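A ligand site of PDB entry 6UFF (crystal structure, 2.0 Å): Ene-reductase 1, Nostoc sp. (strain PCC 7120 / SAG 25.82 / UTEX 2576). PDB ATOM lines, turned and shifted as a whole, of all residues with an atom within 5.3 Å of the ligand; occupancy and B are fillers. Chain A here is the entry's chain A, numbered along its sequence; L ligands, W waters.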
ATOM      1  N   ALA A  62     -16.839 -22.909   2.995  1.00  0.00           N
ATOM      2  CA  ALA A  62     -15.539 -23.097   3.637  1.00  0.00           C
ATOM      3  C   ALA A  62     -14.463 -22.223   2.988  1.00  0.00           C
ATOM      4  O   ALA A  62     -14.546 -21.893   1.801  1.00  0.00           O
ATOM      5  CB  ALA A  62     -15.127 -24.566   3.566  1.00  0.00           C
ATOM      6  N   PRO A  63     -13.444 -21.805   3.771  1.00  0.00           N
ATOM      7  CA  PRO A  63     -12.316 -21.078   3.177  1.00  0.00           C
ATOM      8  C   PRO A  63     -11.554 -21.961   2.209  1.00  0.00           C
ATOM      9  O   PRO A  63     -11.248 -23.113   2.546  1.00  0.00           O
ATOM     10  CB  PRO A  63     -11.463 -20.688   4.388  1.00  0.00           C
ATOM     11  CG  PRO A  63     -11.806 -21.724   5.425  1.00  0.00           C
ATOM     12  CD  PRO A  63     -13.264 -22.051   5.214  1.00  0.00           C
ATOM     13  N   LEU A  64     -11.257 -21.450   1.018  1.00  0.00           N
ATOM     14  CA  LEU A  64     -10.632 -22.258  -0.034  1.00  0.00           C
ATOM     15  C   LEU A  64      -9.542 -21.488  -0.777  1.00  0.00           C
ATOM     16  O   LEU A  64      -9.844 -20.610  -1.591  1.00  0.00           O
ATOM     17  CB  LEU A  64     -11.687 -22.762  -1.019  1.00  0.00           C
ATOM     18  CG  LEU A  64     -12.828 -23.626  -0.487  1.00  0.00           C
ATOM     19  CD1 LEU A  64     -14.067 -23.430  -1.345  1.00  0.00           C
ATOM     20  CD2 LEU A  64     -12.449 -25.099  -0.458  1.00  0.00           C
ATOM     21  N   THR A  65      -8.293 -21.825  -0.491  1.00  0.00           N
ATOM     22  CA  THR A  65      -7.134 -21.321  -1.222  1.00  0.00           C
ATOM     23  C   THR A  65      -7.239 -21.620  -2.719  1.00  0.00           C
ATOM     24  O   THR A  65      -7.331 -22.783  -3.114  1.00  0.00           O
ATOM     25  CB  THR A  65      -5.833 -21.960  -0.670  1.00  0.00           C
ATOM     26  OG1 THR A  65      -5.593 -21.473   0.663  1.00  0.00           O
ATOM     27  CG2 THR A  65      -4.627 -21.633  -1.546  1.00  0.00           C
ATOM     28  N   ARG A  66      -7.242 -20.570  -3.545  1.00  0.00           N
ATOM     29  CA  ARG A  66      -7.354 -20.770  -4.995  1.00  0.00           C
ATOM     30  C   ARG A  66      -6.131 -20.251  -5.761  1.00  0.00           C
ATOM     31  O   ARG A  66      -6.027 -20.479  -6.982  1.00  0.00           O
ATOM     32  CB  ARG A  66      -8.626 -20.081  -5.516  1.00  0.00           C
ATOM     33  CG  ARG A  66      -9.932 -20.525  -4.814  1.00  0.00           C
ATOM     34  CD  ARG A  66     -10.132 -22.041  -4.821  1.00  0.00           C
ATOM     35  NE  ARG A  66     -10.162 -22.588  -6.183  1.00  0.00           N
ATOM     36  CZ  ARG A  66     -11.232 -22.599  -6.969  1.00  0.00           C
ATOM     37  NH1 ARG A  66     -12.382 -22.097  -6.544  1.00  0.00           N
ATOM     38  NH2 ARG A  66     -11.153 -23.120  -8.191  1.00  0.00           N
ATOM     39  N   GLU A  95     -10.829 -17.181   1.396  1.00  0.00           N
ATOM     40  CA  GLU A  95      -9.642 -18.024   1.409  1.00  0.00           C
ATOM     41  C   GLU A  95      -8.634 -17.551   2.437  1.00  0.00           C
ATOM     42  O   GLU A  95      -8.632 -16.379   2.819  1.00  0.00           O
ATOM     43  CB  GLU A  95      -8.993 -18.053   0.026  1.00  0.00           C
ATOM     44  CG  GLU A  95      -8.461 -16.696  -0.403  1.00  0.00           C
ATOM     45  CD  GLU A  95      -8.502 -16.494  -1.903  1.00  0.00           C
ATOM     46  OE1 GLU A  95      -7.551 -16.969  -2.583  1.00  0.00           O
ATOM     47  OE2 GLU A  95      -9.467 -15.869  -2.394  1.00  0.00           O
ATOM     48  N   ALA A  96      -7.776 -18.456   2.877  1.00  0.00           N
ATOM     49  CA  ALA A  96      -6.704 -18.090   3.771  1.00  0.00           C
ATOM     50  C   ALA A  96      -5.889 -16.943   3.164  1.00  0.00           C
ATOM     51  O   ALA A  96      -5.525 -16.993   1.991  1.00  0.00           O
ATOM     52  CB  ALA A  96      -5.823 -19.292   4.072  1.00  0.00           C
ATOM     53  N   GLN A 138     -10.475 -15.095   6.322  1.00  0.00           N
ATOM     54  CA  GLN A 138      -9.673 -15.989   7.143  1.00  0.00           C
ATOM     55  C   GLN A 138      -8.214 -15.497   7.196  1.00  0.00           C
ATOM     56  O   GLN A 138      -7.536 -15.383   6.166  1.00  0.00           O
ATOM     57  CB  GLN A 138      -9.727 -17.446   6.647  1.00  0.00           C
ATOM     58  CG  GLN A 138      -9.069 -18.421   7.632  1.00  0.00           C
ATOM     59  CD  GLN A 138      -8.848 -19.815   7.053  1.00  0.00           C
ATOM     60  OE1 GLN A 138      -8.254 -19.969   5.987  1.00  0.00           O
ATOM     61  NE2 GLN A 138      -9.329 -20.840   7.769  1.00  0.00           N
ATOM     62  N   GLU A 212     -12.022 -14.897  10.501  1.00  0.00           N
ATOM     63  CA  GLU A 212     -11.791 -16.206  11.069  1.00  0.00           C
ATOM     64  C   GLU A 212     -10.298 -16.417  11.287  1.00  0.00           C
ATOM     65  O   GLU A 212      -9.483 -16.222  10.382  1.00  0.00           O
ATOM     66  CB  GLU A 212     -12.354 -17.303  10.164  1.00  0.00           C
ATOM     67  CG  GLU A 212     -11.975 -18.710  10.624  1.00  0.00           C
ATOM     68  CD  GLU A 212     -12.608 -19.795   9.779  1.00  0.00           C
ATOM     69  OE1 GLU A 212     -13.811 -20.084   9.970  1.00  0.00           O
ATOM     70  OE2 GLU A 212     -11.892 -20.364   8.909  1.00  0.00           O
ATOM     71  N   HIS A 214      -7.182 -18.529  11.506  1.00  0.00           N
ATOM     72  CA  HIS A 214      -6.797 -19.826  10.971  1.00  0.00           C
ATOM     73  C   HIS A 214      -5.879 -20.531  11.961  1.00  0.00           C
ATOM     74  O   HIS A 214      -4.665 -20.326  11.959  1.00  0.00           O
ATOM     75  CB  HIS A 214      -6.111 -19.653   9.614  1.00  0.00           C
ATOM     76  CG  HIS A 214      -6.012 -20.922   8.815  1.00  0.00           C
ATOM     77  ND1 HIS A 214      -6.163 -22.170   9.374  1.00  0.00           N
ATOM     78  CD2 HIS A 214      -5.793 -21.123   7.487  1.00  0.00           C
ATOM     79  CE1 HIS A 214      -6.035 -23.092   8.431  1.00  0.00           C
ATOM     80  NE2 HIS A 214      -5.812 -22.475   7.282  1.00  0.00           N
ATOM     81  N   ASN A 217      -4.852 -26.899  10.268  1.00  0.00           N
ATOM     82  CA  ASN A 217      -4.167 -27.413   9.094  1.00  0.00           C
ATOM     83  C   ASN A 217      -2.657 -27.227   9.119  1.00  0.00           C
ATOM     84  O   ASN A 217      -2.004 -27.102   8.077  1.00  0.00           O
ATOM     85  CB  ASN A 217      -4.760 -26.746   7.843  1.00  0.00           C
ATOM     86  CG  ASN A 217      -6.214 -27.138   7.623  1.00  0.00           C
ATOM     87  OD1 ASN A 217      -6.677 -28.132   8.172  1.00  0.00           O
ATOM     88  ND2 ASN A 217      -6.925 -26.366   6.810  1.00  0.00           N
ATOM     89  N   ARG A 266     -10.865 -21.408  13.606  1.00  0.00           N
ATOM     90  CA  ARG A 266     -10.956 -22.700  12.948  1.00  0.00           C
ATOM     91  C   ARG A 266      -9.888 -23.637  13.460  1.00  0.00           C
ATOM     92  O   ARG A 266      -8.724 -23.254  13.586  1.00  0.00           O
ATOM     93  CB  ARG A 266     -10.842 -22.586  11.428  1.00  0.00           C
ATOM     94  CG  ARG A 266     -11.124 -23.931  10.725  1.00  0.00           C
ATOM     95  CD  ARG A 266     -11.203 -23.813   9.217  1.00  0.00           C
ATOM     96  NE  ARG A 266     -12.210 -24.718   8.665  1.00  0.00           N
ATOM     97  CZ  ARG A 266     -12.123 -25.319   7.486  1.00  0.00           C
ATOM     98  NH1 ARG A 266     -11.056 -25.149   6.728  1.00  0.00           N
ATOM     99  NH2 ARG A 266     -13.111 -26.103   7.064  1.00  0.00           N
ATOM    100  N   PHE A 303     -12.832 -28.469  11.246  1.00  0.00           N
ATOM    101  CA  PHE A 303     -12.508 -29.342  10.129  1.00  0.00           C
ATOM    102  C   PHE A 303     -12.373 -30.738  10.722  1.00  0.00           C
ATOM    103  O   PHE A 303     -11.453 -31.000  11.501  1.00  0.00           O
ATOM    104  CB  PHE A 303     -11.207 -28.871   9.452  1.00  0.00           C
ATOM    105  CG  PHE A 303     -10.796 -29.687   8.245  1.00  0.00           C
ATOM    106  CD1 PHE A 303     -11.658 -30.629   7.683  1.00  0.00           C
ATOM    107  CD2 PHE A 303      -9.556 -29.480   7.663  1.00  0.00           C
ATOM    108  CE1 PHE A 303     -11.272 -31.375   6.577  1.00  0.00           C
ATOM    109  CE2 PHE A 303      -9.163 -30.229   6.550  1.00  0.00           C
ATOM    110  CZ  PHE A 303     -10.022 -31.172   6.005  1.00  0.00           C
ATOM    111  N   ASN A 333     -17.484 -29.244   9.368  1.00  0.00           N
ATOM    112  CA  ASN A 333     -17.038 -29.335   7.991  1.00  0.00           C
ATOM    113  C   ASN A 333     -16.329 -30.655   7.719  1.00  0.00           C
ATOM    114  O   ASN A 333     -15.781 -31.269   8.627  1.00  0.00           O
ATOM    115  CB  ASN A 333     -16.119 -28.146   7.666  1.00  0.00           C
ATOM    116  CG  ASN A 333     -15.238 -28.401   6.460  1.00  0.00           C
ATOM    117  OD1 ASN A 333     -14.093 -28.852   6.597  1.00  0.00           O
ATOM    118  ND2 ASN A 333     -15.757 -28.125   5.268  1.00  0.00           N
ATOM    119  N   GLY A 334     -16.358 -31.088   6.461  1.00  0.00           N
ATOM    120  CA  GLY A 334     -15.611 -32.245   6.037  1.00  0.00           C
ATOM    121  C   GLY A 334     -16.517 -33.308   5.448  1.00  0.00           C
ATOM    122  O   GLY A 334     -17.071 -34.134   6.179  1.00  0.00           O
ATOM    123  N   GLY A 335     -16.684 -33.281   4.129  1.00  0.00           N
ATOM    124  CA  GLY A 335     -17.426 -34.309   3.429  1.00  0.00           C
ATOM    125  C   GLY A 335     -18.917 -34.288   3.691  1.00  0.00           C
ATOM    126  O   GLY A 335     -19.593 -35.320   3.596  1.00  0.00           O
ATOM    127  N   TYR A 336     -19.458 -33.114   4.020  1.00  0.00           N
ATOM    128  CA  TYR A 336     -20.878 -33.023   4.313  1.00  0.00           C
ATOM    129  C   TYR A 336     -21.741 -33.043   3.066  1.00  0.00           C
ATOM    130  O   TYR A 336     -21.300 -32.641   1.980  1.00  0.00           O
ATOM    131  CB  TYR A 336     -21.184 -31.773   5.148  1.00  0.00           C
ATOM    132  CG  TYR A 336     -21.003 -32.081   6.606  1.00  0.00           C
ATOM    133  CD1 TYR A 336     -22.033 -32.685   7.328  1.00  0.00           C
ATOM    134  CD2 TYR A 336     -19.800 -31.834   7.248  1.00  0.00           C
ATOM    135  CE1 TYR A 336     -21.868 -32.992   8.659  1.00  0.00           C
ATOM    136  CE2 TYR A 336     -19.627 -32.152   8.578  1.00  0.00           C
ATOM    137  CZ  TYR A 336     -20.667 -32.728   9.291  1.00  0.00           C
ATOM    138  OH  TYR A 336     -20.504 -33.042  10.611  1.00  0.00           O
ATOM    139  N   ALA A 354     -20.280 -26.045   6.961  1.00  0.00           N
ATOM    140  CA  ALA A 354     -19.470 -25.463   5.891  1.00  0.00           C
ATOM    141  C   ALA A 354     -19.132 -26.497   4.818  1.00  0.00           C
ATOM    142  O   ALA A 354     -18.755 -27.621   5.121  1.00  0.00           O
ATOM    143  CB  ALA A 354     -18.198 -24.845   6.454  1.00  0.00           C
ATOM    144  N   PHE A 355     -19.277 -26.111   3.551  1.00  0.00           N
ATOM    145  CA  PHE A 355     -18.902 -26.976   2.448  1.00  0.00           C
ATOM    146  C   PHE A 355     -17.723 -26.340   1.730  1.00  0.00           C
ATOM    147  O   PHE A 355     -17.715 -25.129   1.484  1.00  0.00           O
ATOM    148  CB  PHE A 355     -20.068 -27.185   1.472  1.00  0.00           C
ATOM    149  CG  PHE A 355     -21.270 -27.862   2.075  1.00  0.00           C
ATOM    150  CD1 PHE A 355     -22.162 -27.159   2.872  1.00  0.00           C
ATOM    151  CD2 PHE A 355     -21.514 -29.204   1.824  1.00  0.00           C
ATOM    152  CE1 PHE A 355     -23.276 -27.785   3.432  1.00  0.00           C
ATOM    153  CE2 PHE A 355     -22.637 -29.842   2.368  1.00  0.00           C
ATOM    154  CZ  PHE A 355     -23.516 -29.122   3.169  1.00  0.00           C
ATOM    155  N   GLY A 356     -16.742 -27.159   1.370  1.00  0.00           N
ATOM    156  CA  GLY A 356     -15.591 -26.691   0.621  1.00  0.00           C
ATOM    157  C   GLY A 356     -15.663 -27.059  -0.844  1.00  0.00           C
ATOM    158  O   GLY A 356     -15.993 -26.223  -1.677  1.00  0.00           O
ATOM    159  N   THR A 357     -15.353 -28.319  -1.140  1.00  0.00           N
ATOM    160  CA  THR A 357     -15.322 -28.832  -2.505  1.00  0.00           C
ATOM    161  C   THR A 357     -16.579 -28.475  -3.312  1.00  0.00           C
ATOM    162  O   THR A 357     -16.478 -27.971  -4.432  1.00  0.00           O
ATOM    163  CB  THR A 357     -15.145 -30.368  -2.512  1.00  0.00           C
ATOM    164  OG1 THR A 357     -13.986 -30.710  -1.728  1.00  0.00           O
ATOM    165  CG2 THR A 357     -14.963 -30.891  -3.924  1.00  0.00           C
ATOM    166  N   LEU A 358     -17.745 -28.701  -2.727  1.00  0.00           N
ATOM    167  CA  LEU A 358     -18.991 -28.503  -3.466  1.00  0.00           C
ATOM    168  C   LEU A 358     -19.247 -27.039  -3.817  1.00  0.00           C
ATOM    169  O   LEU A 358     -19.945 -26.749  -4.794  1.00  0.00           O
ATOM    170  CB  LEU A 358     -20.180 -29.069  -2.690  1.00  0.00           C
ATOM    171  CG  LEU A 358     -20.281 -30.599  -2.676  1.00  0.00           C
ATOM    172  CD1 LEU A 358     -21.402 -31.065  -1.761  1.00  0.00           C
ATOM    173  CD2 LEU A 358     -20.493 -31.124  -4.080  1.00  0.00           C
ATOM    174  N   ILE A 360     -16.803 -24.969  -4.655  1.00  0.00           N
ATOM    175  CA  ILE A 360     -15.910 -24.687  -5.770  1.00  0.00           C
ATOM    176  C   ILE A 360     -16.669 -24.866  -7.078  1.00  0.00           C
ATOM    177  O   ILE A 360     -16.644 -24.004  -7.964  1.00  0.00           O
ATOM    178  CB  ILE A 360     -14.674 -25.624  -5.770  1.00  0.00           C
ATOM    179  CG1 ILE A 360     -13.765 -25.278  -4.589  1.00  0.00           C
ATOM    180  CG2 ILE A 360     -13.919 -25.512  -7.096  1.00  0.00           C
ATOM    181  CD1 ILE A 360     -12.584 -26.228  -4.421  1.00  0.00           C
ATOM    182  N   PHE A 383      -8.220 -26.360  -9.107  1.00  0.00           N
ATOM    183  CA  PHE A 383      -8.400 -25.825  -7.754  1.00  0.00           C
ATOM    184  C   PHE A 383      -7.419 -24.694  -7.481  1.00  0.00           C
ATOM    185  O   PHE A 383      -7.798 -23.649  -6.952  1.00  0.00           O
ATOM    186  CB  PHE A 383      -8.238 -26.917  -6.700  1.00  0.00           C
ATOM    187  CG  PHE A 383      -9.414 -27.855  -6.600  1.00  0.00           C
ATOM    188  CD1 PHE A 383     -10.539 -27.669  -7.397  1.00  0.00           C
ATOM    189  CD2 PHE A 383      -9.405 -28.904  -5.699  1.00  0.00           C
ATOM    190  CE1 PHE A 383     -11.624 -28.541  -7.317  1.00  0.00           C
ATOM    191  CE2 PHE A 383     -10.488 -29.769  -5.607  1.00  0.00           C
ATOM    192  CZ  PHE A 383     -11.595 -29.576  -6.418  1.00  0.00           C
ATOM    193  N   TYR A 384      -6.159 -24.886  -7.867  1.00  0.00           N
ATOM    194  CA  TYR A 384      -5.096 -23.931  -7.540  1.00  0.00           C
ATOM    195  C   TYR A 384      -4.509 -23.212  -8.740  1.00  0.00           C
ATOM    196  O   TYR A 384      -4.040 -23.833  -9.691  1.00  0.00           O
ATOM    197  CB  TYR A 384      -3.969 -24.651  -6.795  1.00  0.00           C
ATOM    198  CG  TYR A 384      -4.425 -25.375  -5.549  1.00  0.00           C
ATOM    199  CD1 TYR A 384      -4.872 -24.679  -4.446  1.00  0.00           C
ATOM    200  CD2 TYR A 384      -4.400 -26.767  -5.487  1.00  0.00           C
ATOM    201  CE1 TYR A 384      -5.280 -25.336  -3.300  1.00  0.00           C
ATOM    202  CE2 TYR A 384      -4.801 -27.443  -4.354  1.00  0.00           C
ATOM    203  CZ  TYR A 384      -5.245 -26.717  -3.262  1.00  0.00           C
ATOM    204  OH  TYR A 384      -5.654 -27.382  -2.128  1.00  0.00           O
HETATM  205  N1  LIG L   1      -9.033 -24.730   4.742  1.00  0.00           N
HETATM  206  C1  LIG L   1      -8.659 -23.572   5.385  1.00  0.00           C
HETATM  207  O1  LIG L   1      -8.803 -23.474   6.601  1.00  0.00           O
HETATM  208  N2  LIG L   1      -8.115 -22.522   4.670  1.00  0.00           N
HETATM  209  C2  LIG L   1      -7.954 -22.627   3.303  1.00  0.00           C
HETATM  210  O2  LIG L   1      -7.480 -21.690   2.662  1.00  0.00           O
HETATM  211  C3  LIG L   1      -8.334 -23.798   2.661  1.00  0.00           C
HETATM  212  N3  LIG L   1      -8.170 -23.920   1.304  1.00  0.00           N
HETATM  213  C4  LIG L   1      -8.555 -25.066   0.647  1.00  0.00           C
HETATM  214  C5  LIG L   1      -8.397 -25.154  -0.731  1.00  0.00           C
HETATM  215  C6  LIG L   1      -8.799 -26.301  -1.403  1.00  0.00           C
HETATM  216  C7  LIG L   1      -8.611 -26.393  -2.892  1.00  0.00           C
HETATM  217  C8  LIG L   1      -9.349 -27.363  -0.688  1.00  0.00           C
HETATM  218  C9  LIG L   1      -9.765 -28.615  -1.409  1.00  0.00           C
HETATM  219  C10 LIG L   1      -9.508 -27.267   0.684  1.00  0.00           C
HETATM  220  C11 LIG L   1      -9.113 -26.117   1.363  1.00  0.00           C
HETATM  221  N4  LIG L   1      -9.266 -26.008   2.735  1.00  0.00           N
HETATM  222  C12 LIG L   1      -8.884 -24.845   3.383  1.00  0.00           C
HETATM  223  C13 LIG L   1      -9.908 -27.118   3.518  1.00  0.00           C
HETATM  224  C14 LIG L   1     -11.419 -26.865   3.335  1.00  0.00           C
HETATM  225  O3  LIG L   1     -11.799 -25.588   3.814  1.00  0.00           O
HETATM  226  C15 LIG L   1     -12.330 -27.952   3.915  1.00  0.00           C
HETATM  227  O4  LIG L   1     -12.207 -28.040   5.322  1.00  0.00           O
HETATM  228  C16 LIG L   1     -12.051 -29.292   3.251  1.00  0.00           C
HETATM  229  O5  LIG L   1     -12.102 -29.120   1.840  1.00  0.00           O
HETATM  230  C17 LIG L   1     -13.076 -30.349   3.648  1.00  0.00           C
HETATM  231  O6  LIG L   1     -14.350 -29.831   3.314  1.00  0.00           O
HETATM  232  P1  LIG L   1     -15.177 -30.430   2.067  1.00  0.00           P
HETATM  233  O7  LIG L   1     -15.223 -31.933   2.201  1.00  0.00           O
HETATM  234  O8  LIG L   1     -14.499 -30.039   0.772  1.00  0.00           O
HETATM  235  O9  LIG L   1     -16.580 -29.867   2.076  1.00  0.00           O
HETATM  236  O   HOH W   1     -18.053 -29.849  -0.180  1.00  0.00           O
HETATM  237  O   HOH W   2     -18.081 -30.500   4.374  1.00  0.00           O
HETATM  238  O   HOH W   3      -5.570 -24.506   4.741  1.00  0.00           O
HETATM  239  O   HOH W   4     -16.544 -33.372   0.399  1.00  0.00           O
HETATM  240  O   HOH W   5     -13.508 -33.821   2.193  1.00  0.00           O
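OE1 of Gln 138 lies close to N of Ala 96, at 3.5 Å. The side-chain amide oxygen (OD1) of Asn 333 lies within hydrogen-bond range of the guanidinium group (NH2) of Arg 266, 3.0 Å away. O of Phe 383 lies within hydrogen-bond range of NE of Arg 66, 2.7 Å away. The backbone carbonyl oxygen (O) of Ala 354 sits at hydrogen-bond distance from the side-chain amide nitrogen (ND2) of Asn 333 (3.0 Å). The side-chain amide nitrogen (NE2) of Gln 138 is in hydrogen-bond range of the side-chain carboxylate (OE2) of Glu 212. The backbone carbonyl oxygen of Phe 355 lies within hydrogen-bond range of the backbone NH of Ala 62, at 2.8 Å.
Residues that only touch the ligand: Ala 62 (3.5 Å), Leu 64 (3.3 Å), Phe 303 (3.5 Å), Gly 334 (3.8 Å), Phe 355 (3.7 Å), Phe 383 (3.8 Å) and Tyr 384 (3.2 Å). Within 4 Å of the ligand: Ala 62, Pro 63, Leu 64, Thr 65, Ala 96, Gln 138, His 214, Asn 217, Arg 266, Phe 303, Asn 333, Gly 334, Gly 335, Phe 355, Gly 356, Thr 357, Phe 383 and Tyr 384. Along chain A the residues within 4 Å of the ligand span positions 62 to 384. The nearest printed residue that does not touch the ligand is Ile 360 (4.3 Å).
An oxygen (O2) of the ligand lies close to the backbone NH of Ala 96, 3.3 Å away. N of Gly 335 lies within hydrogen-bond range of O7 of the ligand (2.8 Å). An oxygen (O3) of the ligand sits at hydrogen-bond distance from the backbone carbonyl oxygen of Pro 63 (2.8 Å). N of Thr 65 is in hydrogen-bond range of N3 of the ligand (2.8 Å). The backbone NH of Thr 357 is in hydrogen-bond range of an oxygen (O8) of the ligand (2.7 Å). O9 of the ligand is in hydrogen-bond range of N of Gly 356, at 2.8 Å. NH2 of Arg 266 is in hydrogen-bond range of O4 of the ligand, 2.8 Å away. A nitrogen (N2) of the ligand is in hydrogen-bond range of the side-chain amide oxygen of Gln 138 (2.9 Å). O8 of the ligand is in hydrogen-bond range of OG1 of Thr 357 (2.6 Å). The side-chain amide oxygen (OD1) of Asn 333 sits at hydrogen-bond distance from an oxygen (O4) of the ligand, 2.4 Å away. The side-chain amide nitrogen of Asn 217 lies within hydrogen-bond range of a nitrogen (N1) of the ligand (3.4 Å). An oxygen (O1) of the ligand lies within hydrogen-bond range of a ring nitrogen (NE2) of His 214 (3.2 Å). The side-chain hydroxyl (OG1) of Thr 65 is in hydrogen-bond range of an oxygen (O2) of the ligand, 2.8 Å away.
Water W3 lies within hydrogen-bond range of the side-chain amide nitrogen of Asn 217 (3.1 Å), a nitrogen (N2) of the ligand (3.2 Å) and a ring nitrogen (NE2) of His 214 (3.3 Å).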
